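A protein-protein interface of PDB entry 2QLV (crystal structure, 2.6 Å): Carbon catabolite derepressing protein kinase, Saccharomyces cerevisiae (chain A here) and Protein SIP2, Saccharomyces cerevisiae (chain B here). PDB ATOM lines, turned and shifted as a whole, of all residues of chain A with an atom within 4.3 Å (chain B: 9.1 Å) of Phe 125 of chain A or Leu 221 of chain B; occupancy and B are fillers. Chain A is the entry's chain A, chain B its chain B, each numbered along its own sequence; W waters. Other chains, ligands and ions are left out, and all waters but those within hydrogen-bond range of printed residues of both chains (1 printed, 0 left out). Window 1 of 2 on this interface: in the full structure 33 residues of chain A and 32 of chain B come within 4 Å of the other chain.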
ATOM      1  N   PHE A  48       8.004 -24.430  12.623  1.00  0.00           N
ATOM      2  CA  PHE A  48       6.617 -24.201  12.967  1.00  0.00           C
ATOM      3  C   PHE A  48       6.184 -22.794  12.580  1.00  0.00           C
ATOM      4  O   PHE A  48       6.869 -21.814  12.890  1.00  0.00           O
ATOM      5  CB  PHE A  48       6.419 -24.410  14.464  1.00  0.00           C
ATOM      6  CG  PHE A  48       5.073 -24.939  14.820  1.00  0.00           C
ATOM      7  CD1 PHE A  48       4.698 -26.223  14.426  1.00  0.00           C
ATOM      8  CD2 PHE A  48       4.175 -24.162  15.545  1.00  0.00           C
ATOM      9  CE1 PHE A  48       3.440 -26.730  14.750  1.00  0.00           C
ATOM     10  CE2 PHE A  48       2.909 -24.652  15.879  1.00  0.00           C
ATOM     11  CZ  PHE A  48       2.539 -25.939  15.481  1.00  0.00           C
ATOM     12  N   GLY A  49       5.047 -22.714  11.889  1.00  0.00           N
ATOM     13  CA  GLY A  49       4.495 -21.441  11.457  1.00  0.00           C
ATOM     14  C   GLY A  49       5.459 -20.497  10.763  1.00  0.00           C
ATOM     15  O   GLY A  49       6.137 -20.871   9.808  1.00  0.00           O
ATOM     16  N   ILE A  50       5.505 -19.261  11.248  1.00  0.00           N
ATOM     17  CA  ILE A  50       6.379 -18.244  10.686  1.00  0.00           C
ATOM     18  C   ILE A  50       7.017 -17.394  11.791  1.00  0.00           C
ATOM     19  O   ILE A  50       6.344 -16.990  12.747  1.00  0.00           O
ATOM     20  CB  ILE A  50       5.594 -17.342   9.724  1.00  0.00           C
ATOM     21  CG1 ILE A  50       5.031 -18.188   8.583  1.00  0.00           C
ATOM     22  CG2 ILE A  50       6.491 -16.257   9.168  1.00  0.00           C
ATOM     23  CD1 ILE A  50       4.353 -17.390   7.489  1.00  0.00           C
ATOM     24  N   MET A 109     -10.248 -20.866   9.666  1.00  0.00           N
ATOM     25  CA  MET A 109      -8.820 -20.896   9.928  1.00  0.00           C
ATOM     26  C   MET A 109      -8.611 -20.040  11.160  1.00  0.00           C
ATOM     27  O   MET A 109      -9.449 -19.205  11.480  1.00  0.00           O
ATOM     28  CB  MET A 109      -8.081 -20.308   8.725  1.00  0.00           C
ATOM     29  CG  MET A 109      -6.675 -20.838   8.486  1.00  0.00           C
ATOM     30  SD  MET A 109      -5.968 -20.290   6.886  1.00  0.00           S
ATOM     31  CE  MET A 109      -4.628 -19.191   7.512  1.00  0.00           C
ATOM     32  N   VAL A 110      -7.507 -20.244  11.862  1.00  0.00           N
ATOM     33  CA  VAL A 110      -7.236 -19.462  13.057  1.00  0.00           C
ATOM     34  C   VAL A 110      -5.760 -19.097  13.166  1.00  0.00           C
ATOM     35  O   VAL A 110      -4.890 -19.959  13.083  1.00  0.00           O
ATOM     36  CB  VAL A 110      -7.669 -20.233  14.315  1.00  0.00           C
ATOM     37  CG1 VAL A 110      -7.241 -19.490  15.570  1.00  0.00           C
ATOM     38  CG2 VAL A 110      -9.166 -20.410  14.300  1.00  0.00           C
ATOM     39  N   ILE A 111      -5.474 -17.810  13.345  1.00  0.00           N
ATOM     40  CA  ILE A 111      -4.096 -17.376  13.475  1.00  0.00           C
ATOM     41  C   ILE A 111      -3.806 -16.931  14.899  1.00  0.00           C
ATOM     42  O   ILE A 111      -4.635 -16.298  15.546  1.00  0.00           O
ATOM     43  CB  ILE A 111      -3.770 -16.271  12.471  1.00  0.00           C
ATOM     44  CG1 ILE A 111      -3.936 -16.831  11.055  1.00  0.00           C
ATOM     45  CG2 ILE A 111      -2.357 -15.769  12.689  1.00  0.00           C
ATOM     46  CD1 ILE A 111      -3.293 -16.008   9.976  1.00  0.00           C
ATOM     47  N   VAL A 123       4.125 -16.975  14.241  1.00  0.00           N
ATOM     48  CA  VAL A 123       2.727 -16.897  13.831  1.00  0.00           C
ATOM     49  C   VAL A 123       2.257 -18.292  13.430  1.00  0.00           C
ATOM     50  O   VAL A 123       2.810 -18.915  12.521  1.00  0.00           O
ATOM     51  CB  VAL A 123       2.515 -15.951  12.625  1.00  0.00           C
ATOM     52  CG1 VAL A 123       1.018 -15.798  12.355  1.00  0.00           C
ATOM     53  CG2 VAL A 123       3.156 -14.602  12.896  1.00  0.00           C
ATOM     54  N   ASP A 124       1.230 -18.770  14.116  1.00  0.00           N
ATOM     55  CA  ASP A 124       0.685 -20.083  13.852  1.00  0.00           C
ATOM     56  C   ASP A 124      -0.576 -20.054  12.992  1.00  0.00           C
ATOM     57  O   ASP A 124      -1.485 -19.251  13.208  1.00  0.00           O
ATOM     58  CB  ASP A 124       0.373 -20.780  15.164  1.00  0.00           C
ATOM     59  CG  ASP A 124      -0.320 -22.098  14.957  1.00  0.00           C
ATOM     60  OD1 ASP A 124      -1.120 -22.487  15.835  1.00  0.00           O
ATOM     61  OD2 ASP A 124      -0.058 -22.744  13.915  1.00  0.00           O
ATOM     62  N   PHE A 125      -0.622 -20.954  12.017  1.00  0.00           N
ATOM     63  CA  PHE A 125      -1.760 -21.068  11.122  1.00  0.00           C
ATOM     64  C   PHE A 125      -2.369 -22.435  11.382  1.00  0.00           C
ATOM     65  O   PHE A 125      -1.682 -23.445  11.308  1.00  0.00           O
ATOM     66  CB  PHE A 125      -1.307 -20.974   9.667  1.00  0.00           C
ATOM     67  CG  PHE A 125      -0.386 -19.816   9.382  1.00  0.00           C
ATOM     68  CD1 PHE A 125       0.927 -19.812   9.858  1.00  0.00           C
ATOM     69  CD2 PHE A 125      -0.820 -18.740   8.606  1.00  0.00           C
ATOM     70  CE1 PHE A 125       1.793 -18.756   9.559  1.00  0.00           C
ATOM     71  CE2 PHE A 125       0.037 -17.682   8.302  1.00  0.00           C
ATOM     72  CZ  PHE A 125       1.342 -17.689   8.776  1.00  0.00           C
ATOM     73  N   LYS A 126      -3.656 -22.465  11.700  1.00  0.00           N
ATOM     74  CA  LYS A 126      -4.323 -23.722  11.977  1.00  0.00           C
ATOM     75  C   LYS A 126      -5.635 -23.823  11.238  1.00  0.00           C
ATOM     76  O   LYS A 126      -6.426 -22.890  11.245  1.00  0.00           O
ATOM     77  CB  LYS A 126      -4.594 -23.872  13.474  1.00  0.00           C
ATOM     78  CG  LYS A 126      -5.220 -25.212  13.838  1.00  0.00           C
ATOM     79  CD  LYS A 126      -5.788 -25.236  15.248  1.00  0.00           C
ATOM     80  CE  LYS A 126      -7.095 -24.458  15.330  1.00  0.00           C
ATOM     81  NZ  LYS A 126      -7.683 -24.501  16.701  1.00  0.00           N
ATOM     82  N   PHE A 156      -6.427 -26.112   2.323  1.00  0.00           N
ATOM     83  CA  PHE A 156      -5.838 -25.347   3.411  1.00  0.00           C
ATOM     84  C   PHE A 156      -4.408 -24.872   3.077  1.00  0.00           C
ATOM     85  O   PHE A 156      -4.130 -23.682   3.064  1.00  0.00           O
ATOM     86  CB  PHE A 156      -5.830 -26.206   4.673  1.00  0.00           C
ATOM     87  CG  PHE A 156      -4.990 -25.653   5.785  1.00  0.00           C
ATOM     88  CD1 PHE A 156      -5.318 -24.447   6.393  1.00  0.00           C
ATOM     89  CD2 PHE A 156      -3.866 -26.341   6.224  1.00  0.00           C
ATOM     90  CE1 PHE A 156      -4.530 -23.934   7.431  1.00  0.00           C
ATOM     91  CE2 PHE A 156      -3.074 -25.843   7.254  1.00  0.00           C
ATOM     92  CZ  PHE A 156      -3.406 -24.638   7.858  1.00  0.00           C
ATOM     93  N   LEU A 157      -3.499 -25.801   2.806  1.00  0.00           N
ATOM     94  CA  LEU A 157      -2.124 -25.431   2.486  1.00  0.00           C
ATOM     95  C   LEU A 157      -2.030 -24.453   1.305  1.00  0.00           C
ATOM     96  O   LEU A 157      -1.139 -23.605   1.251  1.00  0.00           O
ATOM     97  CB  LEU A 157      -1.285 -26.691   2.205  1.00  0.00           C
ATOM     98  CG  LEU A 157      -0.903 -27.573   3.404  1.00  0.00           C
ATOM     99  CD1 LEU A 157       0.010 -28.692   2.945  1.00  0.00           C
ATOM    100  CD2 LEU A 157      -0.193 -26.745   4.461  1.00  0.00           C
ATOM    101  N   THR A 160      -3.000 -20.947   2.527  1.00  0.00           N
ATOM    102  CA  THR A 160      -1.981 -20.446   3.429  1.00  0.00           C
ATOM    103  C   THR A 160      -0.774 -20.050   2.605  1.00  0.00           C
ATOM    104  O   THR A 160      -0.004 -19.178   3.000  1.00  0.00           O
ATOM    105  CB  THR A 160      -1.556 -21.502   4.476  1.00  0.00           C
ATOM    106  OG1 THR A 160      -1.026 -22.650   3.808  1.00  0.00           O
ATOM    107  CG2 THR A 160      -2.742 -21.925   5.324  1.00  0.00           C
ATOM    108  N   LEU A 163      -1.486 -16.622   1.154  1.00  0.00           N
ATOM    109  CA  LEU A 163      -1.373 -15.647   2.230  1.00  0.00           C
ATOM    110  C   LEU A 163       0.058 -15.311   2.622  1.00  0.00           C
ATOM    111  O   LEU A 163       0.314 -14.243   3.170  1.00  0.00           O
ATOM    112  CB  LEU A 163      -2.132 -16.138   3.467  1.00  0.00           C
ATOM    113  CG  LEU A 163      -1.838 -15.377   4.764  1.00  0.00           C
ATOM    114  CD1 LEU A 163      -2.258 -13.917   4.621  1.00  0.00           C
ATOM    115  CD2 LEU A 163      -2.569 -16.045   5.916  1.00  0.00           C
ATOM    116  N   ILE A 164       0.988 -16.221   2.360  1.00  0.00           N
ATOM    117  CA  ILE A 164       2.381 -15.968   2.708  1.00  0.00           C
ATOM    118  C   ILE A 164       3.026 -15.101   1.639  1.00  0.00           C
ATOM    119  O   ILE A 164       3.730 -14.135   1.943  1.00  0.00           O
ATOM    120  CB  ILE A 164       3.172 -17.289   2.859  1.00  0.00           C
ATOM    121  CG1 ILE A 164       2.635 -18.062   4.067  1.00  0.00           C
ATOM    122  CG2 ILE A 164       4.657 -17.002   3.032  1.00  0.00           C
ATOM    123  CD1 ILE A 164       3.364 -19.347   4.358  1.00  0.00           C
ATOM    124  N   VAL B 217      -0.806 -33.663  18.525  1.00  0.00           N
ATOM    125  CA  VAL B 217      -1.087 -32.264  18.788  1.00  0.00           C
ATOM    126  C   VAL B 217      -0.798 -31.318  17.616  1.00  0.00           C
ATOM    127  O   VAL B 217      -0.396 -30.169  17.825  1.00  0.00           O
ATOM    128  CB  VAL B 217      -0.312 -31.803  20.048  1.00  0.00           C
ATOM    129  CG1 VAL B 217      -0.545 -32.785  21.186  1.00  0.00           C
ATOM    130  CG2 VAL B 217       1.164 -31.709  19.757  1.00  0.00           C
ATOM    131  N   LEU B 218      -0.999 -31.795  16.386  1.00  0.00           N
ATOM    132  CA  LEU B 218      -0.777 -30.959  15.203  1.00  0.00           C
ATOM    133  C   LEU B 218      -1.740 -31.161  14.028  1.00  0.00           C
ATOM    134  O   LEU B 218      -2.294 -32.243  13.821  1.00  0.00           O
ATOM    135  CB  LEU B 218       0.661 -31.093  14.711  1.00  0.00           C
ATOM    136  CG  LEU B 218       1.705 -30.435  15.617  1.00  0.00           C
ATOM    137  CD1 LEU B 218       2.048 -31.345  16.765  1.00  0.00           C
ATOM    138  CD2 LEU B 218       2.958 -30.144  14.815  1.00  0.00           C
ATOM    139  N   ASN B 219      -1.919 -30.073  13.281  1.00  0.00           N
ATOM    140  CA  ASN B 219      -2.781 -29.964  12.097  1.00  0.00           C
ATOM    141  C   ASN B 219      -2.632 -28.488  11.695  1.00  0.00           C
ATOM    142  O   ASN B 219      -3.514 -27.866  11.090  1.00  0.00           O
ATOM    143  CB  ASN B 219      -4.234 -30.279  12.458  1.00  0.00           C
ATOM    144  CG  ASN B 219      -5.136 -30.362  11.242  1.00  0.00           C
ATOM    145  OD1 ASN B 219      -6.191 -30.996  11.279  1.00  0.00           O
ATOM    146  ND2 ASN B 219      -4.731 -29.715  10.162  1.00  0.00           N
ATOM    147  N   HIS B 220      -1.478 -27.948  12.073  1.00  0.00           N
ATOM    148  CA  HIS B 220      -1.112 -26.570  11.834  1.00  0.00           C
ATOM    149  C   HIS B 220      -0.325 -26.401  10.554  1.00  0.00           C
ATOM    150  O   HIS B 220      -0.452 -27.184   9.614  1.00  0.00           O
ATOM    151  CB  HIS B 220      -0.273 -26.058  12.998  1.00  0.00           C
ATOM    152  CG  HIS B 220      -0.958 -26.162  14.319  1.00  0.00           C
ATOM    153  ND1 HIS B 220      -1.897 -27.131  14.593  1.00  0.00           N
ATOM    154  CD2 HIS B 220      -0.816 -25.442  15.454  1.00  0.00           C
ATOM    155  CE1 HIS B 220      -2.307 -27.004  15.841  1.00  0.00           C
ATOM    156  NE2 HIS B 220      -1.664 -25.986  16.386  1.00  0.00           N
ATOM    157  N   LEU B 221       0.493 -25.361  10.530  1.00  0.00           N
ATOM    158  CA  LEU B 221       1.295 -25.067   9.368  1.00  0.00           C
ATOM    159  C   LEU B 221       2.776 -25.172   9.690  1.00  0.00           C
ATOM    160  O   LEU B 221       3.265 -24.638  10.692  1.00  0.00           O
ATOM    161  CB  LEU B 221       0.985 -23.659   8.855  1.00  0.00           C
ATOM    162  CG  LEU B 221       1.691 -23.266   7.557  1.00  0.00           C
ATOM    163  CD1 LEU B 221       1.037 -24.002   6.399  1.00  0.00           C
ATOM    164  CD2 LEU B 221       1.610 -21.772   7.341  1.00  0.00           C
ATOM    165  N   VAL B 222       3.485 -25.893   8.836  1.00  0.00           N
ATOM    166  CA  VAL B 222       4.912 -26.042   8.988  1.00  0.00           C
ATOM    167  C   VAL B 222       5.487 -25.451   7.723  1.00  0.00           C
ATOM    168  O   VAL B 222       5.097 -25.830   6.615  1.00  0.00           O
ATOM    169  CB  VAL B 222       5.326 -27.506   9.124  1.00  0.00           C
ATOM    170  CG1 VAL B 222       6.756 -27.685   8.625  1.00  0.00           C
ATOM    171  CG2 VAL B 222       5.233 -27.927  10.587  1.00  0.00           C
ATOM    172  N   THR B 223       6.395 -24.499   7.900  1.00  0.00           N
ATOM    173  CA  THR B 223       7.019 -23.829   6.775  1.00  0.00           C
ATOM    174  C   THR B 223       8.515 -24.081   6.814  1.00  0.00           C
ATOM    175  O   THR B 223       9.036 -24.638   7.783  1.00  0.00           O
ATOM    176  CB  THR B 223       6.768 -22.313   6.831  1.00  0.00           C
ATOM    177  OG1 THR B 223       7.473 -21.759   7.946  1.00  0.00           O
ATOM    178  CG2 THR B 223       5.275 -22.022   7.002  1.00  0.00           C
ATOM    179  N   SER B 224       9.193 -23.679   5.745  1.00  0.00           N
ATOM    180  CA  SER B 224      10.637 -23.833   5.631  1.00  0.00           C
ATOM    181  C   SER B 224      11.170 -22.638   4.851  1.00  0.00           C
ATOM    182  O   SER B 224      10.396 -21.883   4.260  1.00  0.00           O
ATOM    183  CB  SER B 224      10.985 -25.143   4.912  1.00  0.00           C
ATOM    184  OG  SER B 224      10.437 -25.179   3.607  1.00  0.00           O
ATOM    185  N   LEU B 231       8.113 -22.117  -3.102  1.00  0.00           N
ATOM    186  CA  LEU B 231       7.844 -22.177  -1.659  1.00  0.00           C
ATOM    187  C   LEU B 231       7.469 -23.591  -1.160  1.00  0.00           C
ATOM    188  O   LEU B 231       6.699 -24.309  -1.798  1.00  0.00           O
ATOM    189  CB  LEU B 231       6.728 -21.190  -1.318  1.00  0.00           C
ATOM    190  CG  LEU B 231       6.400 -20.937   0.150  1.00  0.00           C
ATOM    191  CD1 LEU B 231       7.662 -20.585   0.906  1.00  0.00           C
ATOM    192  CD2 LEU B 231       5.383 -19.810   0.254  1.00  0.00           C
ATOM    193  N   CYS B 232       8.014 -23.978  -0.011  1.00  0.00           N
ATOM    194  CA  CYS B 232       7.775 -25.302   0.563  1.00  0.00           C
ATOM    195  C   CYS B 232       6.919 -25.186   1.820  1.00  0.00           C
ATOM    196  O   CYS B 232       7.357 -24.646   2.828  1.00  0.00           O
ATOM    197  CB  CYS B 232       9.120 -25.965   0.905  1.00  0.00           C
ATOM    198  SG  CYS B 232       9.157 -27.781   0.868  1.00  0.00           S
ATOM    199  N   VAL B 233       5.696 -25.704   1.750  1.00  0.00           N
ATOM    200  CA  VAL B 233       4.761 -25.640   2.872  1.00  0.00           C
ATOM    201  C   VAL B 233       4.195 -27.024   3.192  1.00  0.00           C
ATOM    202  O   VAL B 233       4.104 -27.881   2.309  1.00  0.00           O
ATOM    203  CB  VAL B 233       3.605 -24.653   2.557  1.00  0.00           C
ATOM    204  CG1 VAL B 233       2.638 -25.260   1.560  1.00  0.00           C
ATOM    205  CG2 VAL B 233       2.905 -24.266   3.827  1.00  0.00           C
ATOM    206  N   ALA B 234       3.812 -27.254   4.445  1.00  0.00           N
ATOM    207  CA  ALA B 234       3.296 -28.573   4.819  1.00  0.00           C
ATOM    208  C   ALA B 234       2.461 -28.610   6.082  1.00  0.00           C
ATOM    209  O   ALA B 234       2.600 -27.774   6.960  1.00  0.00           O
ATOM    210  CB  ALA B 234       4.456 -29.561   4.958  1.00  0.00           C
ATOM    211  N   SER B 235       1.602 -29.611   6.172  1.00  0.00           N
ATOM    212  CA  SER B 235       0.761 -29.777   7.347  1.00  0.00           C
ATOM    213  C   SER B 235       0.660 -31.267   7.696  1.00  0.00           C
ATOM    214  O   SER B 235       0.630 -32.129   6.808  1.00  0.00           O
ATOM    215  CB  SER B 235      -0.630 -29.187   7.096  1.00  0.00           C
ATOM    216  OG  SER B 235      -1.363 -29.150   8.300  1.00  0.00           O
ATOM    217  N   ILE B 236       0.630 -31.560   8.994  1.00  0.00           N
ATOM    218  CA  ILE B 236       0.539 -32.937   9.464  1.00  0.00           C
ATOM    219  C   ILE B 236      -0.914 -33.328   9.624  1.00  0.00           C
ATOM    220  O   ILE B 236      -1.648 -32.731  10.405  1.00  0.00           O
ATOM    221  CB  ILE B 236       1.236 -33.127  10.803  1.00  0.00           C
ATOM    222  CG1 ILE B 236       2.699 -32.710  10.692  1.00  0.00           C
ATOM    223  CG2 ILE B 236       1.145 -34.580  11.223  1.00  0.00           C
ATOM    224  CD1 ILE B 236       3.411 -32.710  12.020  1.00  0.00           C
ATOM    225  N   GLN B 246       1.891 -33.918   4.845  1.00  0.00           N
ATOM    226  CA  GLN B 246       1.648 -33.492   3.472  1.00  0.00           C
ATOM    227  C   GLN B 246       2.483 -32.252   3.224  1.00  0.00           C
ATOM    228  O   GLN B 246       2.391 -31.276   3.965  1.00  0.00           O
ATOM    229  CB  GLN B 246       0.166 -33.153   3.270  1.00  0.00           C
ATOM    230  CG  GLN B 246      -0.785 -34.191   3.834  1.00  0.00           C
ATOM    231  CD  GLN B 246      -1.437 -35.042   2.763  1.00  0.00           C
ATOM    232  OE1 GLN B 246      -0.768 -35.728   1.981  1.00  0.00           O
ATOM    233  NE2 GLN B 246      -2.766 -35.003   2.725  1.00  0.00           N
ATOM    234  N   ILE B 247       3.301 -32.299   2.185  1.00  0.00           N
ATOM    235  CA  ILE B 247       4.150 -31.181   1.842  1.00  0.00           C
ATOM    236  C   ILE B 247       3.775 -30.681   0.469  1.00  0.00           C
ATOM    237  O   ILE B 247       3.855 -31.422  -0.520  1.00  0.00           O
ATOM    238  CB  ILE B 247       5.616 -31.598   1.813  1.00  0.00           C
ATOM    239  CG1 ILE B 247       6.019 -32.162   3.174  1.00  0.00           C
ATOM    240  CG2 ILE B 247       6.472 -30.412   1.436  1.00  0.00           C
ATOM    241  CD1 ILE B 247       7.120 -33.201   3.092  1.00  0.00           C
ATOM    242  N   LEU B 248       3.369 -29.419   0.411  1.00  0.00           N
ATOM    243  CA  LEU B 248       2.984 -28.779  -0.848  1.00  0.00           C
ATOM    244  C   LEU B 248       4.079 -27.855  -1.387  1.00  0.00           C
ATOM    245  O   LEU B 248       4.513 -26.945  -0.693  1.00  0.00           O
ATOM    246  CB  LEU B 248       1.724 -27.967  -0.624  1.00  0.00           C
ATOM    247  CG  LEU B 248       1.163 -27.266  -1.841  1.00  0.00           C
ATOM    248  CD1 LEU B 248       1.074 -28.227  -3.027  1.00  0.00           C
ATOM    249  CD2 LEU B 248      -0.196 -26.746  -1.460  1.00  0.00           C
HETATM  250  O   HOH W   1       1.804 -22.872  12.123  1.00  0.00           O
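Water W1 lies within hydrogen-bond range of the side-chain carboxylate of Asp 124 of chain A (2.6 Å), the backbone carbonyl oxygen of Leu 221 of chain B (2.7 Å), the backbone NH of Phe 125 of chain A (3.1 Å) and the backbone NH of Gly 49 of chain A (3.3 Å).
Among the printed residues, merely in contact across the chains: Phe 48 of chain A with Leu 218 of chain B (3.4 Å), Phe 48 of chain A with His 220 of chain B (3.4 Å), Phe 48 of chain A with Leu 221 of chain B (3.9 Å), Asp 124 of chain A with His 220 of chain B (3.0 Å), Phe 125 of chain A with His 220 of chain B (3.2 Å), Lys 126 of chain A with His 220 of chain B (3.9 Å), Phe 156 of chain A with His 220 of chain B (3.8 Å), Phe 156 of chain A with Ser 235 of chain B (3.9 Å), Leu 157 of chain A with Leu 221 of chain B (3.6 Å), Leu 157 of chain A with Ala 234 of chain B (3.6 Å), Leu 157 of chain A with Ser 235 of chain B (3.6 Å), Leu 157 of chain A with Gln 246 of chain B (3.7 Å), Leu 157 of chain A with Leu 248 of chain B (3.8 Å) and Thr 160 of chain A with Leu 221 of chain B (3.6 Å).
Of the 17 printed residues of chain B, 8 touch a printed residue of chain A. Hydrophobic or aromatic side chains of chain B that line the printed part of chain A: Leu 218, His 220, Leu 221 and Leu 248. Of the 15 printed residues of chain A, 8 touch a printed residue of chain B. Printed residues of chain A that touch a printed residue of chain B: Phe 48, Gly 49, Asp 124, Phe 125, Lys 126, Phe 156, Leu 157 and Thr 160. Hydrophobic or aromatic side chains of chain A within 4 Å of the printed part of chain B: Phe 48, Phe 125, Phe 156 and Leu 157. Among the printed residues, 17 pairs touch across the chains.
OG1 of Thr 160 of chain A sits at hydrogen-bond distance from O of Leu 157 of chain A, at 2.7 Å. The side-chain hydroxyl of Thr 160 of chain A sits close to the backbone carbonyl oxygen of Phe 156 of chain A (3.4 Å). O of Val 233 of chain B sits at hydrogen-bond distance from N of Leu 248 of chain B (2.6 Å). O of His 220 of chain B sits at hydrogen-bond distance from OG of Ser 235 of chain B, at 2.5 Å. The backbone NH (N) of Val 222 of chain B is in hydrogen-bond range of the backbone carbonyl oxygen (O) of Ala 234 of chain B. The backbone carbonyl oxygen (O) of Lys 126 of chain A is in hydrogen-bond range of the backbone NH (N) of Val 110 of chain A.
Of chain B, only His 220 (3.2 Å) and Leu 221 (3.0 Å) come within 4 Å of Phe 125 of chain A. Of the printed residues of chain A, His 220 of chain B touches Phe 48, Asp 124, Phe 125, Lys 126 and Phe 156. Leu 221 of chain B touches just these residues of chain A: Phe 48, Gly 49, Phe 125, Leu 157 and Thr 160. Printed residues of chain A within 4 Å of Ala 234 of chain B: Leu 157 (3.6 Å). Of the printed residues of chain A, Ser 235 of chain B touches Phe 156 and Leu 157. Of the printed residues of chain A, Leu 248 of chain B touches Leu 157. The nearest residue of chain B that does not touch Phe 125 of chain A is Asn 219 of chain B (4.8 Å).
The backbone NH of Gly 49 of chain A lies within hydrogen-bond range of the backbone carbonyl oxygen of Leu 221 of chain B. O of Phe 125 of chain A lies within hydrogen-bond range of N of Leu 221 of chain B, 3.0 Å away. OG1 of Thr 223 of chain B lies within hydrogen-bond range of O of Gly 49 of chain A, at 2.5 Å.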
